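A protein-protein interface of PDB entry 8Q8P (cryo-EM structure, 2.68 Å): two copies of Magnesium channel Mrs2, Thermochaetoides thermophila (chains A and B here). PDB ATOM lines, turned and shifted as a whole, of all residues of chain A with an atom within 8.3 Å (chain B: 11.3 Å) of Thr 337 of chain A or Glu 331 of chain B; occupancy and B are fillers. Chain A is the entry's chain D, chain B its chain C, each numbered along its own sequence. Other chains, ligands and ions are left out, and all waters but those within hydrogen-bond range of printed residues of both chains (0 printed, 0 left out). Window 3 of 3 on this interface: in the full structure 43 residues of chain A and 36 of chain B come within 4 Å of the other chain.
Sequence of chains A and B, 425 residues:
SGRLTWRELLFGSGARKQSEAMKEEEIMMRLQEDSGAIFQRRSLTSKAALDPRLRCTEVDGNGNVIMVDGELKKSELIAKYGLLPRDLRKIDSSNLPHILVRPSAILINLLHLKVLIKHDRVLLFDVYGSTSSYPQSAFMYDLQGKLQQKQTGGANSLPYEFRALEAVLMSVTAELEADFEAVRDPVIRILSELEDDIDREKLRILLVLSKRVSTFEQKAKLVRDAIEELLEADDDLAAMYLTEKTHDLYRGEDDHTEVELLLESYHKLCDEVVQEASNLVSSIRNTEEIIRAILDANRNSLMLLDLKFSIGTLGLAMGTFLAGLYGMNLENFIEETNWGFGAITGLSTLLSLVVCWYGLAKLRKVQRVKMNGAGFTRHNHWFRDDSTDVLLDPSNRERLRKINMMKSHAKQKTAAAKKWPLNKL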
ATOM      1  N   ASN A 332     -10.575 -13.033  24.883  1.00  0.00           N
ATOM      2  CA  ASN A 332     -11.718 -13.868  24.542  1.00  0.00           C
ATOM      3  C   ASN A 332     -12.375 -13.487  23.223  1.00  0.00           C
ATOM      4  O   ASN A 332     -13.263 -14.213  22.765  1.00  0.00           O
ATOM      5  CB  ASN A 332     -12.766 -13.817  25.664  1.00  0.00           C
ATOM      6  CG  ASN A 332     -13.041 -12.404  26.144  1.00  0.00           C
ATOM      7  OD1 ASN A 332     -12.694 -11.432  25.476  1.00  0.00           O
ATOM      8  ND2 ASN A 332     -13.665 -12.287  27.310  1.00  0.00           N
ATOM      9  N   PHE A 333     -11.978 -12.368  22.617  1.00  0.00           N
ATOM     10  CA  PHE A 333     -12.419 -11.885  21.309  1.00  0.00           C
ATOM     11  C   PHE A 333     -13.884 -11.463  21.279  1.00  0.00           C
ATOM     12  O   PHE A 333     -14.350 -10.987  20.236  1.00  0.00           O
ATOM     13  CB  PHE A 333     -12.185 -12.916  20.195  1.00  0.00           C
ATOM     14  CG  PHE A 333     -10.780 -13.444  20.140  1.00  0.00           C
ATOM     15  CD1 PHE A 333      -9.775 -12.718  19.525  1.00  0.00           C
ATOM     16  CD2 PHE A 333     -10.466 -14.671  20.700  1.00  0.00           C
ATOM     17  CE1 PHE A 333      -8.483 -13.203  19.473  1.00  0.00           C
ATOM     18  CE2 PHE A 333      -9.177 -15.162  20.653  1.00  0.00           C
ATOM     19  CZ  PHE A 333      -8.183 -14.427  20.037  1.00  0.00           C
ATOM     20  N   ILE A 334     -14.627 -11.618  22.374  1.00  0.00           N
ATOM     21  CA  ILE A 334     -16.036 -11.240  22.402  1.00  0.00           C
ATOM     22  C   ILE A 334     -16.308 -10.363  23.617  1.00  0.00           C
ATOM     23  O   ILE A 334     -17.447 -10.271  24.088  1.00  0.00           O
ATOM     24  CB  ILE A 334     -16.949 -12.481  22.405  1.00  0.00           C
ATOM     25  CG1 ILE A 334     -16.587 -13.409  23.567  1.00  0.00           C
ATOM     26  CG2 ILE A 334     -16.856 -13.218  21.077  1.00  0.00           C
ATOM     27  CD1 ILE A 334     -17.456 -14.644  23.651  1.00  0.00           C
ATOM     28  N   GLU A 335     -15.262  -9.712  24.132  1.00  0.00           N
ATOM     29  CA  GLU A 335     -15.424  -8.871  25.313  1.00  0.00           C
ATOM     30  C   GLU A 335     -16.227  -7.611  25.009  1.00  0.00           C
ATOM     31  O   GLU A 335     -17.015  -7.163  25.851  1.00  0.00           O
ATOM     32  CB  GLU A 335     -14.055  -8.503  25.886  1.00  0.00           C
ATOM     33  CG  GLU A 335     -14.114  -7.662  27.150  1.00  0.00           C
ATOM     34  CD  GLU A 335     -12.764  -7.537  27.828  1.00  0.00           C
ATOM     35  OE1 GLU A 335     -11.818  -8.237  27.407  1.00  0.00           O
ATOM     36  OE2 GLU A 335     -12.648  -6.740  28.783  1.00  0.00           O
ATOM     37  N   GLU A 336     -16.048  -7.032  23.824  1.00  0.00           N
ATOM     38  CA  GLU A 336     -16.726  -5.794  23.464  1.00  0.00           C
ATOM     39  C   GLU A 336     -18.060  -6.017  22.767  1.00  0.00           C
ATOM     40  O   GLU A 336     -18.743  -5.039  22.445  1.00  0.00           O
ATOM     41  CB  GLU A 336     -15.821  -4.938  22.570  1.00  0.00           C
ATOM     42  CG  GLU A 336     -14.471  -4.582  23.184  1.00  0.00           C
ATOM     43  CD  GLU A 336     -14.542  -3.409  24.149  1.00  0.00           C
ATOM     44  OE1 GLU A 336     -15.453  -3.379  25.003  1.00  0.00           O
ATOM     45  OE2 GLU A 336     -13.680  -2.511  24.051  1.00  0.00           O
ATOM     46  N   THR A 337     -18.448  -7.266  22.525  1.00  0.00           N
ATOM     47  CA  THR A 337     -19.723  -7.544  21.883  1.00  0.00           C
ATOM     48  C   THR A 337     -20.875  -7.312  22.860  1.00  0.00           C
ATOM     49  O   THR A 337     -20.692  -7.224  24.078  1.00  0.00           O
ATOM     50  CB  THR A 337     -19.757  -8.978  21.354  1.00  0.00           C
ATOM     51  OG1 THR A 337     -19.553  -9.893  22.438  1.00  0.00           O
ATOM     52  CG2 THR A 337     -18.672  -9.186  20.310  1.00  0.00           C
ATOM     53  N   ASN A 338     -22.083  -7.214  22.305  1.00  0.00           N
ATOM     54  CA  ASN A 338     -23.292  -6.995  23.087  1.00  0.00           C
ATOM     55  C   ASN A 338     -24.139  -8.258  23.216  1.00  0.00           C
ATOM     56  O   ASN A 338     -25.325  -8.171  23.549  1.00  0.00           O
ATOM     57  CB  ASN A 338     -24.119  -5.865  22.473  1.00  0.00           C
ATOM     58  CG  ASN A 338     -24.471  -6.121  21.020  1.00  0.00           C
ATOM     59  OD1 ASN A 338     -23.713  -5.772  20.115  1.00  0.00           O
ATOM     60  ND2 ASN A 338     -25.627  -6.732  20.789  1.00  0.00           N
ATOM     61  N   TRP A 339     -23.553  -9.427  22.959  1.00  0.00           N
ATOM     62  CA  TRP A 339     -24.282 -10.685  23.056  1.00  0.00           C
ATOM     63  C   TRP A 339     -23.524 -11.790  23.775  1.00  0.00           C
ATOM     64  O   TRP A 339     -24.102 -12.863  23.979  1.00  0.00           O
ATOM     65  CB  TRP A 339     -24.669 -11.185  21.656  1.00  0.00           C
ATOM     66  CG  TRP A 339     -23.517 -11.220  20.698  1.00  0.00           C
ATOM     67  CD1 TRP A 339     -23.150 -10.240  19.823  1.00  0.00           C
ATOM     68  CD2 TRP A 339     -22.577 -12.288  20.520  1.00  0.00           C
ATOM     69  NE1 TRP A 339     -22.043 -10.631  19.110  1.00  0.00           N
ATOM     70  CE2 TRP A 339     -21.672 -11.884  19.519  1.00  0.00           C
ATOM     71  CE3 TRP A 339     -22.416 -13.546  21.109  1.00  0.00           C
ATOM     72  CZ2 TRP A 339     -20.620 -12.692  19.094  1.00  0.00           C
ATOM     73  CZ3 TRP A 339     -21.370 -14.347  20.686  1.00  0.00           C
ATOM     74  CH2 TRP A 339     -20.486 -13.917  19.689  1.00  0.00           C
ATOM     75  N   GLY A 340     -22.265 -11.580  24.161  1.00  0.00           N
ATOM     76  CA  GLY A 340     -21.498 -12.653  24.771  1.00  0.00           C
ATOM     77  C   GLY A 340     -21.997 -13.043  26.150  1.00  0.00           C
ATOM     78  O   GLY A 340     -22.023 -14.226  26.497  1.00  0.00           O
ATOM     79  N   PHE A 341     -22.397 -12.055  26.955  1.00  0.00           N
ATOM     80  CA  PHE A 341     -22.781 -12.328  28.338  1.00  0.00           C
ATOM     81  C   PHE A 341     -23.990 -13.254  28.405  1.00  0.00           C
ATOM     82  O   PHE A 341     -23.963 -14.286  29.089  1.00  0.00           O
ATOM     83  CB  PHE A 341     -23.065 -11.012  29.064  1.00  0.00           C
ATOM     84  CG  PHE A 341     -23.272 -11.165  30.544  1.00  0.00           C
ATOM     85  CD1 PHE A 341     -22.191 -11.199  31.407  1.00  0.00           C
ATOM     86  CD2 PHE A 341     -24.548 -11.266  31.073  1.00  0.00           C
ATOM     87  CE1 PHE A 341     -22.376 -11.338  32.769  1.00  0.00           C
ATOM     88  CE2 PHE A 341     -24.741 -11.405  32.434  1.00  0.00           C
ATOM     89  CZ  PHE A 341     -23.652 -11.440  33.283  1.00  0.00           C
ATOM     90  N   GLY A 342     -25.065 -12.899  27.696  1.00  0.00           N
ATOM     91  CA  GLY A 342     -26.259 -13.725  27.719  1.00  0.00           C
ATOM     92  C   GLY A 342     -26.032 -15.096  27.115  1.00  0.00           C
ATOM     93  O   GLY A 342     -26.550 -16.099  27.615  1.00  0.00           O
ATOM     94  N   ALA A 343     -25.247 -15.162  26.038  1.00  0.00           N
ATOM     95  CA  ALA A 343     -24.959 -16.445  25.404  1.00  0.00           C
ATOM     96  C   ALA A 343     -24.196 -17.364  26.350  1.00  0.00           C
ATOM     97  O   ALA A 343     -24.518 -18.552  26.474  1.00  0.00           O
ATOM     98  CB  ALA A 343     -24.173 -16.227  24.112  1.00  0.00           C
ATOM     99  N   THR A 345     -24.065 -17.171  29.674  1.00  0.00           N
ATOM    100  CA  THR A 345     -24.936 -17.531  30.789  1.00  0.00           C
ATOM    101  C   THR A 345     -25.906 -18.638  30.389  1.00  0.00           C
ATOM    102  O   THR A 345     -26.105 -19.608  31.133  1.00  0.00           O
ATOM    103  CB  THR A 345     -25.697 -16.299  31.280  1.00  0.00           C
ATOM    104  OG1 THR A 345     -24.763 -15.275  31.647  1.00  0.00           O
ATOM    105  CG2 THR A 345     -26.554 -16.648  32.487  1.00  0.00           C
ATOM    106  N   LEU B 325     -20.815 -15.530  38.054  1.00  0.00           N
ATOM    107  CA  LEU B 325     -21.354 -15.203  36.737  1.00  0.00           C
ATOM    108  C   LEU B 325     -21.038 -13.764  36.344  1.00  0.00           C
ATOM    109  O   LEU B 325     -20.764 -13.479  35.173  1.00  0.00           O
ATOM    110  CB  LEU B 325     -22.863 -15.440  36.706  1.00  0.00           C
ATOM    111  CG  LEU B 325     -23.345 -16.839  36.326  1.00  0.00           C
ATOM    112  CD1 LEU B 325     -24.862 -16.885  36.307  1.00  0.00           C
ATOM    113  CD2 LEU B 325     -22.778 -17.251  34.977  1.00  0.00           C
ATOM    114  N   TYR B 326     -21.077 -12.843  37.304  1.00  0.00           N
ATOM    115  CA  TYR B 326     -20.817 -11.434  37.037  1.00  0.00           C
ATOM    116  C   TYR B 326     -19.336 -11.082  37.065  1.00  0.00           C
ATOM    117  O   TYR B 326     -18.986  -9.921  36.827  1.00  0.00           O
ATOM    118  CB  TYR B 326     -21.573 -10.558  38.040  1.00  0.00           C
ATOM    119  CG  TYR B 326     -22.960 -10.174  37.579  1.00  0.00           C
ATOM    120  CD1 TYR B 326     -23.192  -8.948  36.970  1.00  0.00           C
ATOM    121  CD2 TYR B 326     -24.033 -11.039  37.741  1.00  0.00           C
ATOM    122  CE1 TYR B 326     -24.455  -8.591  36.542  1.00  0.00           C
ATOM    123  CE2 TYR B 326     -25.300 -10.692  37.314  1.00  0.00           C
ATOM    124  CZ  TYR B 326     -25.505  -9.466  36.716  1.00  0.00           C
ATOM    125  OH  TYR B 326     -26.764  -9.112  36.291  1.00  0.00           O
ATOM    126  N   GLY B 327     -18.462 -12.044  37.345  1.00  0.00           N
ATOM    127  CA  GLY B 327     -17.036 -11.817  37.314  1.00  0.00           C
ATOM    128  C   GLY B 327     -16.382 -12.033  35.971  1.00  0.00           C
ATOM    129  O   GLY B 327     -15.164 -11.865  35.851  1.00  0.00           O
ATOM    130  N   MET B 328     -17.152 -12.408  34.953  1.00  0.00           N
ATOM    131  CA  MET B 328     -16.595 -12.622  33.626  1.00  0.00           C
ATOM    132  C   MET B 328     -16.248 -11.292  32.969  1.00  0.00           C
ATOM    133  O   MET B 328     -16.879 -10.264  33.236  1.00  0.00           O
ATOM    134  CB  MET B 328     -17.582 -13.393  32.752  1.00  0.00           C
ATOM    135  CG  MET B 328     -18.066 -14.694  33.366  1.00  0.00           C
ATOM    136  SD  MET B 328     -19.138 -15.635  32.264  1.00  0.00           S
ATOM    137  CE  MET B 328     -20.486 -14.480  32.030  1.00  0.00           C
ATOM    138  N   ASN B 329     -15.236 -11.316  32.101  1.00  0.00           N
ATOM    139  CA  ASN B 329     -14.799 -10.119  31.382  1.00  0.00           C
ATOM    140  C   ASN B 329     -15.677  -9.926  30.144  1.00  0.00           C
ATOM    141  O   ASN B 329     -15.256 -10.089  28.997  1.00  0.00           O
ATOM    142  CB  ASN B 329     -13.326 -10.225  31.017  1.00  0.00           C
ATOM    143  CG  ASN B 329     -12.430 -10.311  32.236  1.00  0.00           C
ATOM    144  OD1 ASN B 329     -12.730  -9.738  33.282  1.00  0.00           O
ATOM    145  ND2 ASN B 329     -11.323 -11.030  32.106  1.00  0.00           N
ATOM    146  N   LEU B 330     -16.933  -9.571  30.402  1.00  0.00           N
ATOM    147  CA  LEU B 330     -17.916  -9.339  29.351  1.00  0.00           C
ATOM    148  C   LEU B 330     -18.676  -8.060  29.687  1.00  0.00           C
ATOM    149  O   LEU B 330     -18.327  -7.335  30.623  1.00  0.00           O
ATOM    150  CB  LEU B 330     -18.847 -10.551  29.201  1.00  0.00           C
ATOM    151  CG  LEU B 330     -18.193 -11.858  28.745  1.00  0.00           C
ATOM    152  CD1 LEU B 330     -19.173 -13.015  28.826  1.00  0.00           C
ATOM    153  CD2 LEU B 330     -17.646 -11.717  27.335  1.00  0.00           C
ATOM    154  N   GLU B 331     -19.724  -7.780  28.915  1.00  0.00           N
ATOM    155  CA  GLU B 331     -20.537  -6.581  29.092  1.00  0.00           C
ATOM    156  C   GLU B 331     -21.774  -6.945  29.905  1.00  0.00           C
ATOM    157  O   GLU B 331     -22.614  -7.729  29.453  1.00  0.00           O
ATOM    158  CB  GLU B 331     -20.922  -5.983  27.741  1.00  0.00           C
ATOM    159  CG  GLU B 331     -21.725  -4.695  27.834  1.00  0.00           C
ATOM    160  CD  GLU B 331     -20.904  -3.527  28.347  1.00  0.00           C
ATOM    161  OE1 GLU B 331     -19.662  -3.573  28.229  1.00  0.00           O
ATOM    162  OE2 GLU B 331     -21.502  -2.563  28.867  1.00  0.00           O
ATOM    163  N   ASN B 332     -21.885  -6.373  31.105  1.00  0.00           N
ATOM    164  CA  ASN B 332     -23.024  -6.611  31.979  1.00  0.00           C
ATOM    165  C   ASN B 332     -24.022  -5.461  32.003  1.00  0.00           C
ATOM    166  O   ASN B 332     -25.096  -5.612  32.598  1.00  0.00           O
ATOM    167  CB  ASN B 332     -22.545  -6.896  33.411  1.00  0.00           C
ATOM    168  CG  ASN B 332     -21.488  -5.914  33.879  1.00  0.00           C
ATOM    169  OD1 ASN B 332     -21.305  -4.852  33.285  1.00  0.00           O
ATOM    170  ND2 ASN B 332     -20.785  -6.267  34.948  1.00  0.00           N
ATOM    171  N   PHE B 333     -23.692  -4.323  31.392  1.00  0.00           N
ATOM    172  CA  PHE B 333     -24.546  -3.148  31.227  1.00  0.00           C
ATOM    173  C   PHE B 333     -24.858  -2.434  32.537  1.00  0.00           C
ATOM    174  O   PHE B 333     -25.528  -1.394  32.510  1.00  0.00           O
ATOM    175  CB  PHE B 333     -25.870  -3.479  30.524  1.00  0.00           C
ATOM    176  CG  PHE B 333     -25.702  -4.223  29.229  1.00  0.00           C
ATOM    177  CD1 PHE B 333     -25.381  -3.548  28.064  1.00  0.00           C
ATOM    178  CD2 PHE B 333     -25.869  -5.596  29.179  1.00  0.00           C
ATOM    179  CE1 PHE B 333     -25.228  -4.230  26.871  1.00  0.00           C
ATOM    180  CE2 PHE B 333     -25.717  -6.284  27.991  1.00  0.00           C
ATOM    181  CZ  PHE B 333     -25.396  -5.600  26.836  1.00  0.00           C
ATOM    182  N   ILE B 334     -24.405  -2.946  33.681  1.00  0.00           N
ATOM    183  CA  ILE B 334     -24.679  -2.313  34.966  1.00  0.00           C
ATOM    184  C   ILE B 334     -23.381  -2.151  35.745  1.00  0.00           C
ATOM    185  O   ILE B 334     -23.392  -2.045  36.978  1.00  0.00           O
ATOM    186  CB  ILE B 334     -25.710  -3.118  35.778  1.00  0.00           C
ATOM    187  CG1 ILE B 334     -25.247  -4.566  35.948  1.00  0.00           C
ATOM    188  CG2 ILE B 334     -27.077  -3.064  35.112  1.00  0.00           C
ATOM    189  CD1 ILE B 334     -26.199  -5.418  36.757  1.00  0.00           C
ATOM    190  N   GLU B 335     -22.252  -2.130  35.033  1.00  0.00           N
ATOM    191  CA  GLU B 335     -20.960  -2.006  35.699  1.00  0.00           C
ATOM    192  C   GLU B 335     -20.760  -0.620  36.301  1.00  0.00           C
ATOM    193  O   GLU B 335     -20.169  -0.497  37.379  1.00  0.00           O
ATOM    194  CB  GLU B 335     -19.833  -2.326  34.717  1.00  0.00           C
ATOM    195  CG  GLU B 335     -18.441  -2.269  35.323  1.00  0.00           C
ATOM    196  CD  GLU B 335     -17.380  -2.839  34.403  1.00  0.00           C
ATOM    197  OE1 GLU B 335     -17.746  -3.425  33.362  1.00  0.00           O
ATOM    198  OE2 GLU B 335     -16.180  -2.702  34.720  1.00  0.00           O
ATOM    199  N   GLU B 336     -21.244   0.424  35.631  1.00  0.00           N
ATOM    200  CA  GLU B 336     -21.052   1.790  36.097  1.00  0.00           C
ATOM    201  C   GLU B 336     -22.178   2.285  36.995  1.00  0.00           C
ATOM    202  O   GLU B 336     -22.107   3.419  37.480  1.00  0.00           O
ATOM    203  CB  GLU B 336     -20.902   2.739  34.901  1.00  0.00           C
ATOM    204  CG  GLU B 336     -19.757   2.393  33.955  1.00  0.00           C
ATOM    205  CD  GLU B 336     -18.404   2.879  34.447  1.00  0.00           C
ATOM    206  OE1 GLU B 336     -18.084   2.682  35.638  1.00  0.00           O
ATOM    207  OE2 GLU B 336     -17.655   3.463  33.636  1.00  0.00           O
ATOM    208  N   THR B 337     -23.206   1.473  37.229  1.00  0.00           N
ATOM    209  CA  THR B 337     -24.300   1.880  38.096  1.00  0.00           C
ATOM    210  C   THR B 337     -23.862   1.843  39.560  1.00  0.00           C
ATOM    211  O   THR B 337     -22.845   1.247  39.924  1.00  0.00           O
ATOM    212  CB  THR B 337     -25.517   0.979  37.886  1.00  0.00           C
ATOM    213  OG1 THR B 337     -25.160  -0.380  38.162  1.00  0.00           O
ATOM    214  CG2 THR B 337     -26.015   1.085  36.452  1.00  0.00           C
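Positions printed for both chains: 332, 333, 334, 335, 336 and 337. Of the 9 pairs that touch across the chains among the printed residues, none has its exchanged pair printed and touching as well.
The side-chain amide oxygen of Asn 332 of chain A sits close to the backbone NH of Glu 335 of chain A, 3.4 Å away. The backbone carbonyl oxygen (O) of Ile 334 of chain A is in hydrogen-bond range of the side-chain hydroxyl (OG1) of Thr 337 of chain A (2.7 Å). The backbone carbonyl oxygen (O) of Phe 341 of chain A lies within hydrogen-bond range of the side-chain hydroxyl (OG1) of Thr 345 of chain A, 2.9 Å away.
Of the 13 printed residues of chain B, 5 touch a printed residue of chain A. Hydrophobic or aromatic side chains of chain B that line the printed part of chain A: Met 328 and Leu 330. Printed residues of chain A that touch a printed residue of chain B: Asn 332, Ile 334, Glu 335, Thr 337, Gly 340 and Phe 341. Among the printed residues, no Asp or Glu carboxylate lies within 4 Å of a Lys or Arg side-chain nitrogen of the other chain.
Of the printed residues of chain B, Asn 332 of chain A touches Asn 329 (3.2 Å). Phe 333 of chain A touches none of the printed residues of chain B. Glu 336 of chain A touches none of the printed residues of chain B. Of chain B, only Glu 331 comes within 4 Å of Thr 337 of chain A. No residue of chain B comes within 4 Å of Trp 339 of chain A. Of chain B, only Leu 330 (3.9 Å) comes within 4 Å of Gly 340 of chain A. Of chain B, only Leu 325 (3.6 Å), Met 328 (3.7 Å), Leu 330 (3.7 Å) and Glu 331 (3.3 Å) come within 4 Å of Phe 341 of chain A. Of the printed residues of chain A, Leu 325 of chain B touches Phe 341 (3.6 Å). Glu 331 of chain B touches just these residues of chain A: Thr 337 and Phe 341. Glu 335 of chain B touches none of the printed residues of chain A. The nearest residue of chain B that does not touch Thr 337 of chain A is Leu 330 of chain B (5.6 Å). The nearest printed residue of chain A that does not touch Asn 329 of chain B is Ile 334 of chain A (5.4 Å).
The side-chain amide nitrogen of Asn 332 of chain A lies within hydrogen-bond range of the backbone carbonyl oxygen of Asn 329 of chain B, at 3.2 Å.
Ile 334 of chain A touches Leu 330 of chain B (O to CD2, 3.6 Å). Glu 335 of chain A touches Asn 329 of chain B (CG to O, 3.3 Å). Thr 337 of chain A touches Glu 331 of chain B. Gly 340 of chain A touches Leu 330 of chain B. CE1 of Phe 341 of chain A touches O of Leu 325 of chain B, 3.6 Å away. CE1 of Phe 341 of chain A touches CE of Met 328 of chain B, at 3.7 Å. Phe 341 of chain A touches Leu 330 of chain B (CA to CD1, 3.7 Å). Glu 331 of chain B touches Phe 341 of chain A.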
